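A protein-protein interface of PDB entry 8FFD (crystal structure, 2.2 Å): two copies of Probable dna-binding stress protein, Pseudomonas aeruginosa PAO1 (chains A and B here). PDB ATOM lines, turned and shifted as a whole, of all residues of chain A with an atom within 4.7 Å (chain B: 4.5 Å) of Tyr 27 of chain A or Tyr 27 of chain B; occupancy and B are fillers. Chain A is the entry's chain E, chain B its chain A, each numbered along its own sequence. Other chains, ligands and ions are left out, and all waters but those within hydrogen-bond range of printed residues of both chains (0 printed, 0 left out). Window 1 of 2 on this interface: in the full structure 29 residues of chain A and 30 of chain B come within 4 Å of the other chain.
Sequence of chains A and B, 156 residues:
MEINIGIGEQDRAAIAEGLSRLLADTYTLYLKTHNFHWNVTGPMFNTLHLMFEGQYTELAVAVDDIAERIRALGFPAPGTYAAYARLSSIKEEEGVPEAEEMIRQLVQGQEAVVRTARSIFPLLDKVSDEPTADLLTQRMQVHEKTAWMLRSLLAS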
ATOM      1  N   LEU A  23      11.488   6.478   7.715  1.00  0.00           N
ATOM      2  CA  LEU A  23      10.441   6.478   6.702  1.00  0.00           C
ATOM      3  C   LEU A  23       9.524   7.681   6.873  1.00  0.00           C
ATOM      4  O   LEU A  23       9.103   8.290   5.886  1.00  0.00           O
ATOM      5  CB  LEU A  23       9.653   5.157   6.748  1.00  0.00           C
ATOM      6  CG  LEU A  23       8.433   5.050   5.840  1.00  0.00           C
ATOM      7  CD1 LEU A  23       8.842   5.235   4.409  1.00  0.00           C
ATOM      8  CD2 LEU A  23       7.721   3.717   6.025  1.00  0.00           C
ATOM      9  N   ALA A  24       9.208   8.052   8.115  1.00  0.00           N
ATOM     10  CA  ALA A  24       8.326   9.201   8.302  1.00  0.00           C
ATOM     11  C   ALA A  24       9.022  10.504   7.915  1.00  0.00           C
ATOM     12  O   ALA A  24       8.388  11.413   7.372  1.00  0.00           O
ATOM     13  CB  ALA A  24       7.825   9.266   9.745  1.00  0.00           C
ATOM     14  N   ASP A  25      10.317  10.627   8.208  1.00  0.00           N
ATOM     15  CA  ASP A  25      11.049  11.813   7.776  1.00  0.00           C
ATOM     16  C   ASP A  25      11.166  11.860   6.253  1.00  0.00           C
ATOM     17  O   ASP A  25      10.969  12.916   5.642  1.00  0.00           O
ATOM     18  CB  ASP A  25      12.432  11.844   8.410  1.00  0.00           C
ATOM     19  CG  ASP A  25      12.386  12.100   9.912  1.00  0.00           C
ATOM     20  OD1 ASP A  25      11.334  12.537  10.387  1.00  0.00           O
ATOM     21  OD2 ASP A  25      13.400  11.859  10.608  1.00  0.00           O
ATOM     22  N   THR A  26      11.520  10.723   5.632  1.00  0.00           N
ATOM     23  CA  THR A  26      11.646  10.653   4.181  1.00  0.00           C
ATOM     24  C   THR A  26      10.321  10.977   3.513  1.00  0.00           C
ATOM     25  O   THR A  26      10.279  11.744   2.548  1.00  0.00           O
ATOM     26  CB  THR A  26      12.136   9.271   3.744  1.00  0.00           C
ATOM     27  OG1 THR A  26      13.412   9.011   4.321  1.00  0.00           O
ATOM     28  CG2 THR A  26      12.327   9.208   2.230  1.00  0.00           C
ATOM     29  N   TYR A  27       9.224  10.469   4.061  1.00  0.00           N
ATOM     30  CA  TYR A  27       7.927  10.716   3.455  1.00  0.00           C
ATOM     31  C   TYR A  27       7.476  12.155   3.661  1.00  0.00           C
ATOM     32  O   TYR A  27       6.881  12.753   2.755  1.00  0.00           O
ATOM     33  CB  TYR A  27       6.871   9.756   4.009  1.00  0.00           C
ATOM     34  CG  TYR A  27       5.693   9.652   3.068  1.00  0.00           C
ATOM     35  CD1 TYR A  27       4.694  10.618   3.069  1.00  0.00           C
ATOM     36  CD2 TYR A  27       5.613   8.637   2.142  1.00  0.00           C
ATOM     37  CE1 TYR A  27       3.638  10.555   2.198  1.00  0.00           C
ATOM     38  CE2 TYR A  27       4.525   8.556   1.241  1.00  0.00           C
ATOM     39  CZ  TYR A  27       3.553   9.517   1.275  1.00  0.00           C
ATOM     40  OH  TYR A  27       2.499   9.439   0.392  1.00  0.00           O
ATOM     41  N   THR A  28       7.681  12.720   4.858  1.00  0.00           N
ATOM     42  CA  THR A  28       7.339  14.129   5.038  1.00  0.00           C
ATOM     43  C   THR A  28       8.163  15.000   4.089  1.00  0.00           C
ATOM     44  O   THR A  28       7.632  15.905   3.433  1.00  0.00           O
ATOM     45  CB  THR A  28       7.546  14.540   6.493  1.00  0.00           C
ATOM     46  OG1 THR A  28       6.761  13.698   7.336  1.00  0.00           O
ATOM     47  CG2 THR A  28       7.118  15.989   6.719  1.00  0.00           C
ATOM     48  N   LEU A  29       9.451  14.707   3.959  1.00  0.00           N
ATOM     49  CA  LEU A  29      10.277  15.453   3.016  1.00  0.00           C
ATOM     50  C   LEU A  29       9.787  15.262   1.581  1.00  0.00           C
ATOM     51  O   LEU A  29       9.819  16.198   0.773  1.00  0.00           O
ATOM     52  CB  LEU A  29      11.723  15.022   3.156  1.00  0.00           C
ATOM     53  CG  LEU A  29      12.727  15.774   2.293  1.00  0.00           C
ATOM     54  CD1 LEU A  29      12.581  17.222   2.552  1.00  0.00           C
ATOM     55  CD2 LEU A  29      14.137  15.284   2.613  1.00  0.00           C
ATOM     56  N   TYR A  30       9.313  14.060   1.257  1.00  0.00           N
ATOM     57  CA  TYR A  30       8.779  13.800  -0.070  1.00  0.00           C
ATOM     58  C   TYR A  30       7.591  14.691  -0.359  1.00  0.00           C
ATOM     59  O   TYR A  30       7.547  15.366  -1.394  1.00  0.00           O
ATOM     60  CB  TYR A  30       8.407  12.330  -0.173  1.00  0.00           C
ATOM     61  CG  TYR A  30       7.489  11.905  -1.308  1.00  0.00           C
ATOM     62  CD1 TYR A  30       7.813  12.133  -2.643  1.00  0.00           C
ATOM     63  CD2 TYR A  30       6.332  11.187  -1.027  1.00  0.00           C
ATOM     64  CE1 TYR A  30       6.961  11.687  -3.673  1.00  0.00           C
ATOM     65  CE2 TYR A  30       5.483  10.749  -2.033  1.00  0.00           C
ATOM     66  CZ  TYR A  30       5.812  10.989  -3.347  1.00  0.00           C
ATOM     67  OH  TYR A  30       4.962  10.523  -4.293  1.00  0.00           O
ATOM     68  N   LEU A  31       6.626  14.730   0.562  1.00  0.00           N
ATOM     69  CA  LEU A  31       5.444  15.552   0.343  1.00  0.00           C
ATOM     70  C   LEU A  31       5.778  17.042   0.323  1.00  0.00           C
ATOM     71  O   LEU A  31       5.191  17.800  -0.459  1.00  0.00           O
ATOM     72  CB  LEU A  31       4.399  15.248   1.406  1.00  0.00           C
ATOM     73  CG  LEU A  31       3.082  15.996   1.306  1.00  0.00           C
ATOM     74  CD1 LEU A  31       2.554  15.890  -0.115  1.00  0.00           C
ATOM     75  CD2 LEU A  31       2.064  15.429   2.292  1.00  0.00           C
ATOM     76  N   VAL A  63      10.964   5.971  -0.323  1.00  0.00           N
ATOM     77  CA  VAL A  63       9.922   5.584   0.624  1.00  0.00           C
ATOM     78  C   VAL A  63       9.595   4.107   0.464  1.00  0.00           C
ATOM     79  O   VAL A  63       9.440   3.368   1.440  1.00  0.00           O
ATOM     80  CB  VAL A  63       8.685   6.481   0.405  1.00  0.00           C
ATOM     81  CG1 VAL A  63       7.436   5.863   0.955  1.00  0.00           C
ATOM     82  CG2 VAL A  63       8.913   7.859   1.031  1.00  0.00           C
ATOM     83  N   TYR A  81      -1.254   9.475   7.521  1.00  0.00           N
ATOM     84  CA  TYR A  81      -0.950  10.838   7.964  1.00  0.00           C
ATOM     85  C   TYR A  81      -0.641  10.871   9.455  1.00  0.00           C
ATOM     86  O   TYR A  81       0.339  11.478   9.888  1.00  0.00           O
ATOM     87  CB  TYR A  81      -2.124  11.774   7.669  1.00  0.00           C
ATOM     88  CG  TYR A  81      -2.530  11.888   6.228  1.00  0.00           C
ATOM     89  CD1 TYR A  81      -1.603  11.804   5.224  1.00  0.00           C
ATOM     90  CD2 TYR A  81      -3.852  12.105   5.886  1.00  0.00           C
ATOM     91  CE1 TYR A  81      -1.962  11.929   3.925  1.00  0.00           C
ATOM     92  CE2 TYR A  81      -4.227  12.207   4.600  1.00  0.00           C
ATOM     93  CZ  TYR A  81      -3.279  12.125   3.616  1.00  0.00           C
ATOM     94  OH  TYR A  81      -3.658  12.242   2.308  1.00  0.00           O
ATOM     95  N   TYR A  84       2.804   9.191  10.317  1.00  0.00           N
ATOM     96  CA  TYR A  84       3.978   9.942   9.899  1.00  0.00           C
ATOM     97  C   TYR A  84       4.082  11.252  10.667  1.00  0.00           C
ATOM     98  O   TYR A  84       5.184  11.716  10.953  1.00  0.00           O
ATOM     99  CB  TYR A  84       3.938  10.230   8.401  1.00  0.00           C
ATOM    100  CG  TYR A  84       4.077   9.028   7.478  1.00  0.00           C
ATOM    101  CD1 TYR A  84       4.622   7.829   7.924  1.00  0.00           C
ATOM    102  CD2 TYR A  84       3.676   9.114   6.149  1.00  0.00           C
ATOM    103  CE1 TYR A  84       4.737   6.743   7.082  1.00  0.00           C
ATOM    104  CE2 TYR A  84       3.797   8.032   5.285  1.00  0.00           C
ATOM    105  CZ  TYR A  84       4.322   6.849   5.754  1.00  0.00           C
ATOM    106  OH  TYR A  84       4.434   5.779   4.891  1.00  0.00           O
ATOM    107  N   LEU B  23      -8.108  16.572  -4.710  1.00  0.00           N
ATOM    108  CA  LEU B  23      -6.706  16.286  -4.453  1.00  0.00           C
ATOM    109  C   LEU B  23      -6.560  15.508  -3.151  1.00  0.00           C
ATOM    110  O   LEU B  23      -5.889  14.469  -3.101  1.00  0.00           O
ATOM    111  CB  LEU B  23      -5.905  17.600  -4.420  1.00  0.00           C
ATOM    112  CG  LEU B  23      -4.409  17.459  -4.098  1.00  0.00           C
ATOM    113  CD1 LEU B  23      -3.795  16.405  -5.005  1.00  0.00           C
ATOM    114  CD2 LEU B  23      -3.646  18.763  -4.272  1.00  0.00           C
ATOM    115  N   ALA B  24      -7.207  15.982  -2.085  1.00  0.00           N
ATOM    116  CA  ALA B  24      -7.043  15.325  -0.789  1.00  0.00           C
ATOM    117  C   ALA B  24      -7.512  13.872  -0.830  1.00  0.00           C
ATOM    118  O   ALA B  24      -6.830  12.976  -0.322  1.00  0.00           O
ATOM    119  CB  ALA B  24      -7.807  16.097   0.287  1.00  0.00           C
ATOM    120  N   ASP B  25      -8.692  13.618  -1.396  1.00  0.00           N
ATOM    121  CA  ASP B  25      -9.160  12.235  -1.507  1.00  0.00           C
ATOM    122  C   ASP B  25      -8.190  11.398  -2.322  1.00  0.00           C
ATOM    123  O   ASP B  25      -7.853  10.269  -1.951  1.00  0.00           O
ATOM    124  CB  ASP B  25     -10.532  12.183  -2.152  1.00  0.00           C
ATOM    125  CG  ASP B  25     -11.592  12.798  -1.296  1.00  0.00           C
ATOM    126  OD1 ASP B  25     -11.294  13.088  -0.127  1.00  0.00           O
ATOM    127  OD2 ASP B  25     -12.718  12.994  -1.799  1.00  0.00           O
ATOM    128  N   THR B  26      -7.745  11.937  -3.449  1.00  0.00           N
ATOM    129  CA  THR B  26      -6.821  11.214  -4.308  1.00  0.00           C
ATOM    130  C   THR B  26      -5.524  10.940  -3.578  1.00  0.00           C
ATOM    131  O   THR B  26      -4.957   9.846  -3.696  1.00  0.00           O
ATOM    132  CB  THR B  26      -6.553  12.017  -5.597  1.00  0.00           C
ATOM    133  OG1 THR B  26      -7.779  12.262  -6.306  1.00  0.00           O
ATOM    134  CG2 THR B  26      -5.630  11.292  -6.495  1.00  0.00           C
ATOM    135  N   TYR B  27      -5.012  11.932  -2.842  1.00  0.00           N
ATOM    136  CA  TYR B  27      -3.750  11.703  -2.145  1.00  0.00           C
ATOM    137  C   TYR B  27      -3.919  10.690  -1.015  1.00  0.00           C
ATOM    138  O   TYR B  27      -3.045   9.847  -0.786  1.00  0.00           O
ATOM    139  CB  TYR B  27      -3.177  13.005  -1.587  1.00  0.00           C
ATOM    140  CG  TYR B  27      -1.712  12.834  -1.324  1.00  0.00           C
ATOM    141  CD1 TYR B  27      -1.247  12.189  -0.175  1.00  0.00           C
ATOM    142  CD2 TYR B  27      -0.788  13.271  -2.244  1.00  0.00           C
ATOM    143  CE1 TYR B  27       0.102  11.992   0.025  1.00  0.00           C
ATOM    144  CE2 TYR B  27       0.561  13.095  -2.052  1.00  0.00           C
ATOM    145  CZ  TYR B  27       0.999  12.459  -0.920  1.00  0.00           C
ATOM    146  OH  TYR B  27       2.337  12.284  -0.769  1.00  0.00           O
ATOM    147  N   THR B  28      -5.010  10.784  -0.268  1.00  0.00           N
ATOM    148  CA  THR B  28      -5.227   9.818   0.801  1.00  0.00           C
ATOM    149  C   THR B  28      -5.341   8.411   0.229  1.00  0.00           C
ATOM    150  O   THR B  28      -4.681   7.477   0.702  1.00  0.00           O
ATOM    151  CB  THR B  28      -6.457  10.236   1.593  1.00  0.00           C
ATOM    152  OG1 THR B  28      -6.211  11.552   2.117  1.00  0.00           O
ATOM    153  CG2 THR B  28      -6.748   9.280   2.730  1.00  0.00           C
ATOM    154  N   LEU B  29      -6.137   8.249  -0.826  1.00  0.00           N
ATOM    155  CA  LEU B  29      -6.197   6.965  -1.513  1.00  0.00           C
ATOM    156  C   LEU B  29      -4.820   6.525  -1.989  1.00  0.00           C
ATOM    157  O   LEU B  29      -4.483   5.337  -1.923  1.00  0.00           O
ATOM    158  CB  LEU B  29      -7.165   7.057  -2.689  1.00  0.00           C
ATOM    159  CG  LEU B  29      -7.265   5.834  -3.574  1.00  0.00           C
ATOM    160  CD1 LEU B  29      -7.530   4.630  -2.698  1.00  0.00           C
ATOM    161  CD2 LEU B  29      -8.389   6.044  -4.555  1.00  0.00           C
ATOM    162  N   TYR B  30      -4.005   7.466  -2.470  1.00  0.00           N
ATOM    163  CA  TYR B  30      -2.655   7.119  -2.904  1.00  0.00           C
ATOM    164  C   TYR B  30      -1.875   6.501  -1.754  1.00  0.00           C
ATOM    165  O   TYR B  30      -1.246   5.441  -1.906  1.00  0.00           O
ATOM    166  CB  TYR B  30      -1.971   8.371  -3.458  1.00  0.00           C
ATOM    167  CG  TYR B  30      -0.485   8.325  -3.669  1.00  0.00           C
ATOM    168  CD1 TYR B  30       0.105   7.294  -4.345  1.00  0.00           C
ATOM    169  CD2 TYR B  30       0.317   9.379  -3.247  1.00  0.00           C
ATOM    170  CE1 TYR B  30       1.479   7.278  -4.551  1.00  0.00           C
ATOM    171  CE2 TYR B  30       1.663   9.379  -3.448  1.00  0.00           C
ATOM    172  CZ  TYR B  30       2.246   8.329  -4.103  1.00  0.00           C
ATOM    173  OH  TYR B  30       3.601   8.319  -4.301  1.00  0.00           O
ATOM    174  N   LEU B  31      -1.914   7.143  -0.583  1.00  0.00           N
ATOM    175  CA  LEU B  31      -1.142   6.642   0.557  1.00  0.00           C
ATOM    176  C   LEU B  31      -1.698   5.311   1.060  1.00  0.00           C
ATOM    177  O   LEU B  31      -0.932   4.388   1.341  1.00  0.00           O
ATOM    178  CB  LEU B  31      -1.109   7.678   1.679  1.00  0.00           C
ATOM    179  CG  LEU B  31      -0.292   7.282   2.899  1.00  0.00           C
ATOM    180  CD1 LEU B  31       1.099   6.807   2.536  1.00  0.00           C
ATOM    181  CD2 LEU B  31      -0.221   8.447   3.852  1.00  0.00           C
ATOM    182  N   VAL B  63      -2.172  12.830  -8.667  1.00  0.00           N
ATOM    183  CA  VAL B  63      -2.044  13.928  -7.712  1.00  0.00           C
ATOM    184  C   VAL B  63      -1.344  15.113  -8.364  1.00  0.00           C
ATOM    185  O   VAL B  63      -1.737  16.265  -8.156  1.00  0.00           O
ATOM    186  CB  VAL B  63      -1.325  13.476  -6.426  1.00  0.00           C
ATOM    187  CG1 VAL B  63      -2.079  12.316  -5.771  1.00  0.00           C
ATOM    188  CG2 VAL B  63       0.118  13.111  -6.681  1.00  0.00           C
ATOM    189  N   TYR B  81       0.031  16.867   5.571  1.00  0.00           N
ATOM    190  CA  TYR B  81      -0.821  15.922   6.289  1.00  0.00           C
ATOM    191  C   TYR B  81      -2.044  16.615   6.840  1.00  0.00           C
ATOM    192  O   TYR B  81      -3.173  16.145   6.678  1.00  0.00           O
ATOM    193  CB  TYR B  81      -0.053  15.274   7.436  1.00  0.00           C
ATOM    194  CG  TYR B  81       1.224  14.579   7.026  1.00  0.00           C
ATOM    195  CD1 TYR B  81       1.352  13.963   5.779  1.00  0.00           C
ATOM    196  CD2 TYR B  81       2.294  14.519   7.894  1.00  0.00           C
ATOM    197  CE1 TYR B  81       2.512  13.317   5.431  1.00  0.00           C
ATOM    198  CE2 TYR B  81       3.453  13.882   7.555  1.00  0.00           C
ATOM    199  CZ  TYR B  81       3.562  13.277   6.329  1.00  0.00           C
ATOM    200  OH  TYR B  81       4.740  12.646   6.001  1.00  0.00           O
ATOM    201  N   TYR B  84      -4.557  17.600   3.927  1.00  0.00           N
ATOM    202  CA  TYR B  84      -5.302  16.486   3.354  1.00  0.00           C
ATOM    203  C   TYR B  84      -6.250  15.868   4.380  1.00  0.00           C
ATOM    204  O   TYR B  84      -7.407  15.575   4.051  1.00  0.00           O
ATOM    205  CB  TYR B  84      -4.338  15.451   2.780  1.00  0.00           C
ATOM    206  CG  TYR B  84      -3.538  15.964   1.586  1.00  0.00           C
ATOM    207  CD1 TYR B  84      -3.983  17.037   0.813  1.00  0.00           C
ATOM    208  CD2 TYR B  84      -2.339  15.375   1.244  1.00  0.00           C
ATOM    209  CE1 TYR B  84      -3.250  17.480  -0.279  1.00  0.00           C
ATOM    210  CE2 TYR B  84      -1.601  15.813   0.179  1.00  0.00           C
ATOM    211  CZ  TYR B  84      -2.049  16.871  -0.571  1.00  0.00           C
ATOM    212  OH  TYR B  84      -1.264  17.284  -1.625  1.00  0.00           O
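The side-chain hydroxyl of Tyr 27 of chain B lies within hydrogen-bond range of the side-chain hydroxyl of Tyr 27 of chain A (3.1 Å). OH of Tyr 81 of chain A lies within hydrogen-bond range of OG1 of Thr 28 of chain B (2.7 Å). The side-chain hydroxyl (OH) of Tyr 30 of chain A is in hydrogen-bond range of the side-chain hydroxyl (OH) of Tyr 30 of chain B, 2.6 Å away. The side-chain hydroxyl (OG1) of Thr 28 of chain A sits at hydrogen-bond distance from the side-chain hydroxyl (OH) of Tyr 81 of chain B (2.6 Å).
The backbone carbonyl oxygen (O) of Ala 24 of chain B sits at hydrogen-bond distance from the side-chain hydroxyl (OG1) of Thr 28 of chain B (2.9 Å). The backbone carbonyl oxygen (O) of Ala 24 of chain A sits at hydrogen-bond distance from the side-chain hydroxyl (OG1) of Thr 28 of chain A.
OH of Tyr 27 of chain A touches CE2 of Tyr 30 of chain B, 3.9 Å away. Tyr 27 of chain A touches Leu 31 of chain B. Tyr 27 of chain A touches Tyr 81 of chain B. Tyr 30 of chain A touches Tyr 27 of chain B. Leu 31 of chain A touches Tyr 27 of chain B. Leu 31 of chain A touches Tyr 81 of chain B (CD2 to CE1, 3.8 Å). Tyr 81 of chain A touches Leu 31 of chain B (CD1 to CD2, 3.9 Å). CD1 of Tyr 81 of chain A touches CD1 of Tyr 81 of chain B, 3.7 Å away. CB of Tyr 84 of chain B touches OH of Tyr 81 of chain A (3.3 Å). Tyr 81 of chain B touches Tyr 84 of chain A (OH to CB, 3.5 Å).
Leu 23 of chain A touches none of the printed residues of chain B. Tyr 27 of chain A touches just these residues of chain B: Tyr 27, Tyr 30, Leu 31 and Tyr 81. Leu 29 of chain A touches none of the printed residues of chain B. Of the printed residues of chain B, Tyr 81 of chain A touches Tyr 27 (3.5 Å), Thr 28 (2.7 Å), Leu 31 (3.9 Å), Tyr 81 (3.7 Å) and Tyr 84 (3.3 Å). Printed residues of chain B within 4 Å of Tyr 84 of chain A: Tyr 81 (3.5 Å). Tyr 27 of chain B touches just these residues of chain A: Tyr 27 (3.1 Å), Tyr 30 (3.7 Å), Leu 31 (3.7 Å) and Tyr 81 (3.5 Å). Of the printed residues of chain A, Thr 28 of chain B touches Tyr 81. The nearest printed residue of chain A that does not touch Tyr 27 of chain B is Tyr 84 of chain A (7.5 Å).
Hydrophobic or aromatic side chains of chain B within 4 Å of the printed part of chain A: Tyr 27, Tyr 30, Leu 31, Tyr 81 and Tyr 84. Hydrophobic or aromatic side chains of chain A that line the printed part of chain B: Tyr 27, Tyr 30, Leu 31, Tyr 81 and Tyr 84. Among the printed residues, no Asp or Glu carboxylate lies within 4 Å of a Lys or Arg side-chain nitrogen of the other chain.
Tyr 27 of chain A touches its own counterpart, Tyr 27 of chain B. Tyr 27 of chain A touches Tyr 30 of chain B, and with the chains exchanged Tyr 30 of chain A touches Tyr 27 of chain B. Tyr 27 of chain A touches Tyr 81 of chain B, and with the chains exchanged Tyr 81 of chain A touches Tyr 27 of chain B. Tyr 81 of chain A touches Tyr 84 of chain B, and with the chains exchanged Tyr 84 of chain A touches Tyr 81 of chain B. Positions printed for both chains: 23, 24, 25, 26, 27, 28, 29, 30, 31, 63, 81 and 84. Of the 15 pairs that touch across the chains among the printed residues, 15 have their exchanged pair printed and touching as well.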
